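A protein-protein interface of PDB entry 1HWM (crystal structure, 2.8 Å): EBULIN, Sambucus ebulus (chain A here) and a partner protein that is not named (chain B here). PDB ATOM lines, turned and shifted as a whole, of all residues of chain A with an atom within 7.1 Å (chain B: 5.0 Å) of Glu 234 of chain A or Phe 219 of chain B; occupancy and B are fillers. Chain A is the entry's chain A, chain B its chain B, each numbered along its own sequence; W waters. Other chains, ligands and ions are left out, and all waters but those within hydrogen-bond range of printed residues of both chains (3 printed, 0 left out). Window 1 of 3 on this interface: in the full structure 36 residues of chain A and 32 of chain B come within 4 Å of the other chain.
Water W1 lies within hydrogen-bond range of the side-chain carboxylate (OE2) of Glu 234 of chain A (2.6 Å), the side-chain amino group (NZ) of Lys 238 of chain A (3.2 Å) and the guanidinium group (NH1) of Arg 181 of chain B (3.3 Å). Water W3 lies within hydrogen-bond range of the backbone carbonyl oxygen (O) of Thr 261 of chain B (2.8 Å) and the backbone carbonyl oxygen (O) of Ile 239 of chain A (2.8 Å). Water W2 lies within hydrogen-bond range of O of Asn 220 of chain B (3.0 Å), OH of Tyr 237 of chain A (3.1 Å) and O of Ser 224 of chain B (3.4 Å).
Among the printed residues, merely in contact across the chains: Asn 37 of chain A with Ile 94 of chain B, Ser 212 of chain A with Ile 94 of chain B, Glu 234 of chain A with Ile 94 of chain B, Glu 234 of chain A with Phe 218 of chain B, Tyr 237 of chain A with Phe 219 of chain B, Tyr 237 of chain A with Ser 221 of chain B and Lys 238 of chain A with Leu 177 of chain B.
The backbone carbonyl oxygen (O) of Asn 37 of chain A is in hydrogen-bond range of the side-chain hydroxyl (OG) of Ser 221 of chain B, at 2.6 Å. The side-chain carboxylate (OE2) of Glu 234 of chain A lies within salt-bridge range of the guanidinium group (NH1) of Arg 181 of chain B (3.5 Å). The backbone carbonyl oxygen (O) of Asn 220 of chain B sits at hydrogen-bond distance from the side-chain hydroxyl (OH) of Tyr 237 of chain A. The side-chain hydroxyl (OG1) of Thr 261 of chain B is in hydrogen-bond range of the backbone carbonyl oxygen (O) of Lys 238 of chain A. The backbone carbonyl oxygen of Phe 219 of chain B lies close to the side-chain carboxylate of Glu 234 of chain A (3.5 Å).
O of Ser 212 of chain A lies within hydrogen-bond range of N of Phe 233 of chain A (3.0 Å). The side-chain carboxylate of Glu 234 of chain A lies within salt-bridge range of the side-chain amino group of Lys 238 of chain A, 3.8 Å away. The backbone carbonyl oxygen of Ile 94 of chain B sits at hydrogen-bond distance from the guanidinium group of Arg 181 of chain B, 2.6 Å away. N of Trp 217 of chain B sits at hydrogen-bond distance from O of Arg 181 of chain B (3.1 Å). The backbone NH of Val 226 of chain B lies within hydrogen-bond range of the backbone carbonyl oxygen of Phe 218 of chain B (2.8 Å). The side-chain amide oxygen (OD1) of Asn 220 of chain B lies within hydrogen-bond range of the side-chain hydroxyl (OG) of Ser 221 of chain B (3.2 Å).
Of the printed residues of chain B, Glu 234 of chain A touches Ile 94 (3.5 Å), Arg 181 (3.2 Å), Phe 218 (3.97 Å) and Phe 219 (3.5 Å). Phe 219 of chain B touches just these residues of chain A: Glu 234 and Tyr 237. Of the printed residues of chain B, Ser 212 of chain A touches Ile 94 (3.8 Å). Of the printed residues of chain B, Asn 37 of chain A touches Ile 94 and Ser 221. Printed residues of chain B within 4 Å of Lys 238 of chain A: Leu 177 (3.8 Å) and Thr 261 (3.0 Å). Of the printed residues of chain A, Phe 218 of chain B touches Glu 234 (3.97 Å). Ile 144 of chain B touches none of the printed residues of chain A. The nearest printed residue of chain B that does not touch Lys 238 of chain A is Phe 219 of chain B (4.4 Å).
Hydrophobic or aromatic side chains of chain B within 4 Å of the printed part of chain A: Ile 94, Leu 177, Phe 218 and Phe 219. Hydrophobic or aromatic side chains of chain A within 4 Å of the printed part of chain B: Tyr 237. Among the printed residues, 12 pairs touch across the chains.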
ATOM      1  N   ASN A  37      -2.424  -6.997  22.424  1.00  0.00           N
ATOM      2  CA  ASN A  37      -2.998  -6.947  21.087  1.00  0.00           C
ATOM      3  C   ASN A  37      -2.661  -5.632  20.398  1.00  0.00           C
ATOM      4  O   ASN A  37      -3.396  -5.174  19.527  1.00  0.00           O
ATOM      5  CB  ASN A  37      -4.517  -7.120  21.155  1.00  0.00           C
ATOM      6  CG  ASN A  37      -4.932  -8.573  21.206  1.00  0.00           C
ATOM      7  OD1 ASN A  37      -4.136  -9.467  20.923  1.00  0.00           O
ATOM      8  ND2 ASN A  37      -6.183  -8.823  21.570  1.00  0.00           N
ATOM      9  N   SER A 212      -8.246 -14.355  20.259  1.00  0.00           N
ATOM     10  CA  SER A 212      -9.295 -13.574  19.603  1.00  0.00           C
ATOM     11  C   SER A 212     -10.672 -13.468  20.296  1.00  0.00           C
ATOM     12  O   SER A 212     -11.186 -12.371  20.490  1.00  0.00           O
ATOM     13  CB  SER A 212      -9.485 -14.090  18.146  1.00  0.00           C
ATOM     14  OG  SER A 212     -10.343 -13.236  17.384  1.00  0.00           O
ATOM     15  N   PHE A 214     -13.756 -13.533  23.165  1.00  0.00           N
ATOM     16  CA  PHE A 214     -13.936 -12.992  24.508  1.00  0.00           C
ATOM     17  C   PHE A 214     -14.688 -14.051  25.307  1.00  0.00           C
ATOM     18  O   PHE A 214     -15.502 -14.784  24.744  1.00  0.00           O
ATOM     19  CB  PHE A 214     -14.782 -11.711  24.473  1.00  0.00           C
ATOM     20  CG  PHE A 214     -14.138 -10.559  23.748  1.00  0.00           C
ATOM     21  CD1 PHE A 214     -14.911  -9.502  23.281  1.00  0.00           C
ATOM     22  CD2 PHE A 214     -12.763 -10.522  23.543  1.00  0.00           C
ATOM     23  CE1 PHE A 214     -14.327  -8.429  22.621  1.00  0.00           C
ATOM     24  CE2 PHE A 214     -12.169  -9.454  22.884  1.00  0.00           C
ATOM     25  CZ  PHE A 214     -12.951  -8.406  22.422  1.00  0.00           C
ATOM     26  N   VAL A 230     -20.595  -7.599  20.784  1.00  0.00           N
ATOM     27  CA  VAL A 230     -19.342  -8.020  20.171  1.00  0.00           C
ATOM     28  C   VAL A 230     -18.685  -9.039  21.103  1.00  0.00           C
ATOM     29  O   VAL A 230     -18.578  -8.810  22.309  1.00  0.00           O
ATOM     30  CB  VAL A 230     -18.394  -6.801  19.919  1.00  0.00           C
ATOM     31  CG1 VAL A 230     -19.177  -5.507  20.038  1.00  0.00           C
ATOM     32  CG2 VAL A 230     -17.221  -6.808  20.893  1.00  0.00           C
ATOM     33  N   ASP A 231     -18.267 -10.169  20.541  1.00  0.00           N
ATOM     34  CA  ASP A 231     -17.646 -11.230  21.329  1.00  0.00           C
ATOM     35  C   ASP A 231     -16.193 -11.514  20.964  1.00  0.00           C
ATOM     36  O   ASP A 231     -15.567 -12.392  21.556  1.00  0.00           O
ATOM     37  CB  ASP A 231     -18.459 -12.519  21.191  1.00  0.00           C
ATOM     38  CG  ASP A 231     -19.055 -12.683  19.807  1.00  0.00           C
ATOM     39  OD1 ASP A 231     -20.174 -13.225  19.697  1.00  0.00           O
ATOM     40  OD2 ASP A 231     -18.402 -12.266  18.829  1.00  0.00           O
ATOM     41  N   ASN A 232     -15.654 -10.781  19.995  1.00  0.00           N
ATOM     42  CA  ASN A 232     -14.266 -10.990  19.591  1.00  0.00           C
ATOM     43  C   ASN A 232     -13.540  -9.684  19.311  1.00  0.00           C
ATOM     44  O   ASN A 232     -14.121  -8.737  18.780  1.00  0.00           O
ATOM     45  CB  ASN A 232     -14.198 -11.896  18.360  1.00  0.00           C
ATOM     46  CG  ASN A 232     -14.896 -11.299  17.159  1.00  0.00           C
ATOM     47  OD1 ASN A 232     -14.256 -10.722  16.280  1.00  0.00           O
ATOM     48  ND2 ASN A 232     -16.214 -11.434  17.115  1.00  0.00           N
ATOM     49  N   PHE A 233     -12.261  -9.645  19.669  1.00  0.00           N
ATOM     50  CA  PHE A 233     -11.430  -8.463  19.479  1.00  0.00           C
ATOM     51  C   PHE A 233     -11.686  -7.754  18.154  1.00  0.00           C
ATOM     52  O   PHE A 233     -12.265  -6.669  18.127  1.00  0.00           O
ATOM     53  CB  PHE A 233      -9.950  -8.840  19.584  1.00  0.00           C
ATOM     54  CG  PHE A 233      -9.027  -7.656  19.665  1.00  0.00           C
ATOM     55  CD1 PHE A 233      -8.921  -6.920  20.839  1.00  0.00           C
ATOM     56  CD2 PHE A 233      -8.270  -7.274  18.564  1.00  0.00           C
ATOM     57  CE1 PHE A 233      -8.076  -5.822  20.912  1.00  0.00           C
ATOM     58  CE2 PHE A 233      -7.421  -6.176  18.630  1.00  0.00           C
ATOM     59  CZ  PHE A 233      -7.325  -5.449  19.805  1.00  0.00           C
ATOM     60  N   GLU A 234     -11.255  -8.368  17.057  1.00  0.00           N
ATOM     61  CA  GLU A 234     -11.434  -7.776  15.736  1.00  0.00           C
ATOM     62  C   GLU A 234     -12.769  -7.066  15.625  1.00  0.00           C
ATOM     63  O   GLU A 234     -12.846  -5.949  15.119  1.00  0.00           O
ATOM     64  CB  GLU A 234     -11.326  -8.844  14.652  1.00  0.00           C
ATOM     65  CG  GLU A 234      -9.906  -9.064  14.153  1.00  0.00           C
ATOM     66  CD  GLU A 234      -9.325  -7.838  13.462  1.00  0.00           C
ATOM     67  OE1 GLU A 234      -9.193  -6.780  14.116  1.00  0.00           O
ATOM     68  OE2 GLU A 234      -8.997  -7.937  12.260  1.00  0.00           O
ATOM     69  N   GLU A 235     -13.825  -7.712  16.100  1.00  0.00           N
ATOM     70  CA  GLU A 235     -15.142  -7.103  16.050  1.00  0.00           C
ATOM     71  C   GLU A 235     -15.125  -5.808  16.850  1.00  0.00           C
ATOM     72  O   GLU A 235     -15.491  -4.747  16.346  1.00  0.00           O
ATOM     73  CB  GLU A 235     -16.181  -8.056  16.627  1.00  0.00           C
ATOM     74  CG  GLU A 235     -17.047  -8.695  15.572  1.00  0.00           C
ATOM     75  CD  GLU A 235     -18.404  -9.063  16.104  1.00  0.00           C
ATOM     76  OE1 GLU A 235     -19.391  -8.407  15.714  1.00  0.00           O
ATOM     77  OE2 GLU A 235     -18.481 -10.007  16.916  1.00  0.00           O
ATOM     78  N   LEU A 236     -14.693  -5.905  18.101  1.00  0.00           N
ATOM     79  CA  LEU A 236     -14.616  -4.750  18.982  1.00  0.00           C
ATOM     80  C   LEU A 236     -13.830  -3.622  18.328  1.00  0.00           C
ATOM     81  O   LEU A 236     -14.310  -2.493  18.236  1.00  0.00           O
ATOM     82  CB  LEU A 236     -13.951  -5.146  20.300  1.00  0.00           C
ATOM     83  CG  LEU A 236     -13.640  -4.005  21.268  1.00  0.00           C
ATOM     84  CD1 LEU A 236     -14.935  -3.442  21.823  1.00  0.00           C
ATOM     85  CD2 LEU A 236     -12.758  -4.513  22.390  1.00  0.00           C
ATOM     86  N   TYR A 237     -12.619  -3.931  17.876  1.00  0.00           N
ATOM     87  CA  TYR A 237     -11.774  -2.935  17.229  1.00  0.00           C
ATOM     88  C   TYR A 237     -12.435  -2.351  15.987  1.00  0.00           C
ATOM     89  O   TYR A 237     -12.738  -1.162  15.936  1.00  0.00           O
ATOM     90  CB  TYR A 237     -10.425  -3.547  16.840  1.00  0.00           C
ATOM     91  CG  TYR A 237      -9.530  -2.574  16.106  1.00  0.00           C
ATOM     92  CD1 TYR A 237      -9.175  -1.358  16.687  1.00  0.00           C
ATOM     93  CD2 TYR A 237      -9.070  -2.850  14.819  1.00  0.00           C
ATOM     94  CE1 TYR A 237      -8.388  -0.437  16.006  1.00  0.00           C
ATOM     95  CE2 TYR A 237      -8.279  -1.934  14.127  1.00  0.00           C
ATOM     96  CZ  TYR A 237      -7.946  -0.729  14.727  1.00  0.00           C
ATOM     97  OH  TYR A 237      -7.191   0.196  14.044  1.00  0.00           O
ATOM     98  N   LYS A 238     -12.649  -3.188  14.980  1.00  0.00           N
ATOM     99  CA  LYS A 238     -13.270  -2.744  13.740  1.00  0.00           C
ATOM    100  C   LYS A 238     -14.447  -1.794  13.970  1.00  0.00           C
ATOM    101  O   LYS A 238     -14.645  -0.847  13.210  1.00  0.00           O
ATOM    102  CB  LYS A 238     -13.739  -3.953  12.927  1.00  0.00           C
ATOM    103  CG  LYS A 238     -12.634  -4.631  12.132  1.00  0.00           C
ATOM    104  CD  LYS A 238     -13.124  -5.909  11.472  1.00  0.00           C
ATOM    105  CE  LYS A 238     -12.032  -6.967  11.444  1.00  0.00           C
ATOM    106  NZ  LYS A 238     -12.426  -8.155  10.636  1.00  0.00           N
ATOM    107  N   ILE A 239     -15.216  -2.041  15.028  1.00  0.00           N
ATOM    108  CA  ILE A 239     -16.381  -1.215  15.340  1.00  0.00           C
ATOM    109  C   ILE A 239     -16.044   0.068  16.101  1.00  0.00           C
ATOM    110  O   ILE A 239     -16.561   1.142  15.783  1.00  0.00           O
ATOM    111  CB  ILE A 239     -17.421  -2.019  16.164  1.00  0.00           C
ATOM    112  CG1 ILE A 239     -18.285  -2.863  15.225  1.00  0.00           C
ATOM    113  CG2 ILE A 239     -18.305  -1.077  16.971  1.00  0.00           C
ATOM    114  CD1 ILE A 239     -19.066  -3.950  15.925  1.00  0.00           C
ATOM    115  N   THR A 240     -15.187  -0.047  17.108  1.00  0.00           N
ATOM    116  CA  THR A 240     -14.802   1.101  17.920  1.00  0.00           C
ATOM    117  C   THR A 240     -13.505   1.776  17.474  1.00  0.00           C
ATOM    118  O   THR A 240     -13.420   3.003  17.423  1.00  0.00           O
ATOM    119  CB  THR A 240     -14.645   0.695  19.401  1.00  0.00           C
ATOM    120  OG1 THR A 240     -13.558  -0.227  19.532  1.00  0.00           O
ATOM    121  CG2 THR A 240     -15.918   0.037  19.911  1.00  0.00           C
ATOM    122  N   ILE B  94      -6.035 -13.389  16.664  1.00  0.00           N
ATOM    123  CA  ILE B  94      -6.721 -12.218  16.125  1.00  0.00           C
ATOM    124  C   ILE B  94      -6.583 -12.060  14.612  1.00  0.00           C
ATOM    125  O   ILE B  94      -7.498 -11.569  13.949  1.00  0.00           O
ATOM    126  CB  ILE B  94      -6.222 -10.925  16.805  1.00  0.00           C
ATOM    127  CG1 ILE B  94      -4.709 -10.787  16.620  1.00  0.00           C
ATOM    128  CG2 ILE B  94      -6.580 -10.947  18.284  1.00  0.00           C
ATOM    129  CD1 ILE B  94      -4.117  -9.580  17.316  1.00  0.00           C
ATOM    130  N   ILE B 144     -14.495   2.509   4.355  1.00  0.00           N
ATOM    131  CA  ILE B 144     -13.059   2.425   4.587  1.00  0.00           C
ATOM    132  C   ILE B 144     -12.413   3.784   4.343  1.00  0.00           C
ATOM    133  O   ILE B 144     -12.023   4.110   3.222  1.00  0.00           O
ATOM    134  CB  ILE B 144     -12.401   1.365   3.676  1.00  0.00           C
ATOM    135  CG1 ILE B 144     -13.016  -0.010   3.958  1.00  0.00           C
ATOM    136  CG2 ILE B 144     -10.898   1.321   3.929  1.00  0.00           C
ATOM    137  CD1 ILE B 144     -12.412  -1.140   3.146  1.00  0.00           C
ATOM    138  N   LEU B 177     -16.792  -6.464   5.689  1.00  0.00           N
ATOM    139  CA  LEU B 177     -15.655  -7.114   6.320  1.00  0.00           C
ATOM    140  C   LEU B 177     -16.018  -8.546   6.697  1.00  0.00           C
ATOM    141  O   LEU B 177     -16.436  -8.822   7.822  1.00  0.00           O
ATOM    142  CB  LEU B 177     -15.226  -6.324   7.558  1.00  0.00           C
ATOM    143  CG  LEU B 177     -14.957  -4.837   7.301  1.00  0.00           C
ATOM    144  CD1 LEU B 177     -14.907  -4.079   8.616  1.00  0.00           C
ATOM    145  CD2 LEU B 177     -13.648  -4.682   6.547  1.00  0.00           C
ATOM    146  N   ARG B 181     -11.789 -13.139   6.800  1.00  0.00           N
ATOM    147  CA  ARG B 181     -10.717 -12.156   6.711  1.00  0.00           C
ATOM    148  C   ARG B 181     -10.522 -11.512   5.346  1.00  0.00           C
ATOM    149  O   ARG B 181      -9.465 -10.946   5.069  1.00  0.00           O
ATOM    150  CB  ARG B 181      -9.401 -12.774   7.190  1.00  0.00           C
ATOM    151  CG  ARG B 181      -9.359 -13.033   8.693  1.00  0.00           C
ATOM    152  CD  ARG B 181     -10.167 -11.992   9.462  1.00  0.00           C
ATOM    153  NE  ARG B 181     -10.720 -12.513  10.709  1.00  0.00           N
ATOM    154  CZ  ARG B 181     -10.254 -12.203  11.914  1.00  0.00           C
ATOM    155  NH1 ARG B 181      -9.223 -11.376  12.033  1.00  0.00           N
ATOM    156  NH2 ARG B 181     -10.818 -12.713  13.000  1.00  0.00           N
ATOM    157  N   ILE B 183     -12.075  -8.804   2.297  1.00  0.00           N
ATOM    158  CA  ILE B 183     -12.894  -7.602   2.176  1.00  0.00           C
ATOM    159  C   ILE B 183     -13.605  -7.639   0.829  1.00  0.00           C
ATOM    160  O   ILE B 183     -12.962  -7.741  -0.213  1.00  0.00           O
ATOM    161  CB  ILE B 183     -12.030  -6.327   2.263  1.00  0.00           C
ATOM    162  CG1 ILE B 183     -11.127  -6.399   3.496  1.00  0.00           C
ATOM    163  CG2 ILE B 183     -12.921  -5.099   2.337  1.00  0.00           C
ATOM    164  CD1 ILE B 183      -9.955  -5.445   3.456  1.00  0.00           C
ATOM    165  N   TRP B 217      -6.601 -10.101   4.264  1.00  0.00           N
ATOM    166  CA  TRP B 217      -6.173  -8.879   4.936  1.00  0.00           C
ATOM    167  C   TRP B 217      -6.364  -8.946   6.447  1.00  0.00           C
ATOM    168  O   TRP B 217      -7.265  -9.621   6.942  1.00  0.00           O
ATOM    169  CB  TRP B 217      -6.940  -7.682   4.370  1.00  0.00           C
ATOM    170  CG  TRP B 217      -6.833  -7.569   2.881  1.00  0.00           C
ATOM    171  CD1 TRP B 217      -7.684  -8.093   1.955  1.00  0.00           C
ATOM    172  CD2 TRP B 217      -5.795  -6.906   2.144  1.00  0.00           C
ATOM    173  NE1 TRP B 217      -7.245  -7.803   0.687  1.00  0.00           N
ATOM    174  CE2 TRP B 217      -6.086  -7.074   0.775  1.00  0.00           C
ATOM    175  CE3 TRP B 217      -4.650  -6.190   2.511  1.00  0.00           C
ATOM    176  CZ2 TRP B 217      -5.273  -6.551  -0.234  1.00  0.00           C
ATOM    177  CZ3 TRP B 217      -3.840  -5.668   1.508  1.00  0.00           C
ATOM    178  CH2 TRP B 217      -4.158  -5.853   0.152  1.00  0.00           C
ATOM    179  N   PHE B 218      -5.507  -8.236   7.172  1.00  0.00           N
ATOM    180  CA  PHE B 218      -5.570  -8.205   8.627  1.00  0.00           C
ATOM    181  C   PHE B 218      -5.535  -6.764   9.120  1.00  0.00           C
ATOM    182  O   PHE B 218      -4.552  -6.053   8.916  1.00  0.00           O
ATOM    183  CB  PHE B 218      -4.391  -8.991   9.212  1.00  0.00           C
ATOM    184  CG  PHE B 218      -4.150  -8.739  10.675  1.00  0.00           C
ATOM    185  CD1 PHE B 218      -5.189  -8.841  11.592  1.00  0.00           C
ATOM    186  CD2 PHE B 218      -2.884  -8.398  11.133  1.00  0.00           C
ATOM    187  CE1 PHE B 218      -4.968  -8.609  12.943  1.00  0.00           C
ATOM    188  CE2 PHE B 218      -2.655  -8.164  12.484  1.00  0.00           C
ATOM    189  CZ  PHE B 218      -3.699  -8.268  13.389  1.00  0.00           C
ATOM    190  N   PHE B 219      -6.612  -6.339   9.773  1.00  0.00           N
ATOM    191  CA  PHE B 219      -6.698  -4.978  10.288  1.00  0.00           C
ATOM    192  C   PHE B 219      -5.968  -4.851  11.620  1.00  0.00           C
ATOM    193  O   PHE B 219      -6.535  -5.111  12.680  1.00  0.00           O
ATOM    194  CB  PHE B 219      -8.163  -4.568  10.451  1.00  0.00           C
ATOM    195  CG  PHE B 219      -8.830  -4.193   9.160  1.00  0.00           C
ATOM    196  CD1 PHE B 219      -9.463  -5.160   8.385  1.00  0.00           C
ATOM    197  CD2 PHE B 219      -8.816  -2.878   8.710  1.00  0.00           C
ATOM    198  CE1 PHE B 219     -10.071  -4.823   7.176  1.00  0.00           C
ATOM    199  CE2 PHE B 219      -9.419  -2.532   7.503  1.00  0.00           C
ATOM    200  CZ  PHE B 219     -10.047  -3.507   6.735  1.00  0.00           C
ATOM    201  N   ASN B 220      -4.702  -4.451  11.551  1.00  0.00           N
ATOM    202  CA  ASN B 220      -3.880  -4.288  12.742  1.00  0.00           C
ATOM    203  C   ASN B 220      -4.375  -3.139  13.614  1.00  0.00           C
ATOM    204  O   ASN B 220      -4.816  -2.105  13.110  1.00  0.00           O
ATOM    205  CB  ASN B 220      -2.425  -4.038  12.341  1.00  0.00           C
ATOM    206  CG  ASN B 220      -1.469  -4.197  13.503  1.00  0.00           C
ATOM    207  OD1 ASN B 220      -1.858  -4.079  14.663  1.00  0.00           O
ATOM    208  ND2 ASN B 220      -0.210  -4.467  13.196  1.00  0.00           N
ATOM    209  N   SER B 221      -4.290  -3.327  14.927  1.00  0.00           N
ATOM    210  CA  SER B 221      -4.735  -2.324  15.887  1.00  0.00           C
ATOM    211  C   SER B 221      -3.998  -0.991  15.778  1.00  0.00           C
ATOM    212  O   SER B 221      -4.462   0.018  16.308  1.00  0.00           O
ATOM    213  CB  SER B 221      -4.586  -2.867  17.312  1.00  0.00           C
ATOM    214  OG  SER B 221      -3.428  -3.674  17.425  1.00  0.00           O
ATOM    215  N   SER B 224      -3.137   0.207  10.686  1.00  0.00           N
ATOM    216  CA  SER B 224      -2.763  -0.292   9.370  1.00  0.00           C
ATOM    217  C   SER B 224      -3.491  -1.578   8.990  1.00  0.00           C
ATOM    218  O   SER B 224      -4.029  -2.280   9.846  1.00  0.00           O
ATOM    219  CB  SER B 224      -1.252  -0.530   9.316  1.00  0.00           C
ATOM    220  OG  SER B 224      -0.947  -1.903   9.491  1.00  0.00           O
ATOM    221  N   VAL B 225      -3.511  -1.868   7.694  1.00  0.00           N
ATOM    222  CA  VAL B 225      -4.139  -3.077   7.173  1.00  0.00           C
ATOM    223  C   VAL B 225      -3.013  -3.861   6.508  1.00  0.00           C
ATOM    224  O   VAL B 225      -2.394  -3.378   5.562  1.00  0.00           O
ATOM    225  CB  VAL B 225      -5.222  -2.747   6.126  1.00  0.00           C
ATOM    226  CG1 VAL B 225      -6.188  -3.911   6.001  1.00  0.00           C
ATOM    227  CG2 VAL B 225      -5.962  -1.481   6.521  1.00  0.00           C
ATOM    228  N   VAL B 226      -2.748  -5.066   7.001  1.00  0.00           N
ATOM    229  CA  VAL B 226      -1.658  -5.874   6.464  1.00  0.00           C
ATOM    230  C   VAL B 226      -2.045  -7.088   5.627  1.00  0.00           C
ATOM    231  O   VAL B 226      -3.142  -7.633   5.751  1.00  0.00           O
ATOM    232  CB  VAL B 226      -0.732  -6.376   7.598  1.00  0.00           C
ATOM    233  CG1 VAL B 226       0.716  -6.124   7.233  1.00  0.00           C
ATOM    234  CG2 VAL B 226      -1.075  -5.681   8.902  1.00  0.00           C
ATOM    235  N   THR B 261     -12.084   2.107   9.921  1.00  0.00           N
ATOM    236  CA  THR B 261     -13.308   1.460   9.470  1.00  0.00           C
ATOM    237  C   THR B 261     -14.537   2.076  10.133  1.00  0.00           C
ATOM    238  O   THR B 261     -14.885   1.727  11.260  1.00  0.00           O
ATOM    239  CB  THR B 261     -13.277  -0.052   9.779  1.00  0.00           C
ATOM    240  OG1 THR B 261     -12.692  -0.268  11.069  1.00  0.00           O
ATOM    241  CG2 THR B 261     -12.460  -0.789   8.732  1.00  0.00           C
HETATM  242  O   HOH W   1      -9.398  -8.956   9.865  1.00  0.00           O
HETATM  243  O   HOH W   2      -6.817  -0.996  11.204  1.00  0.00           O
HETATM  244  O   HOH W   3     -16.931   2.092  13.138  1.00  0.00           O
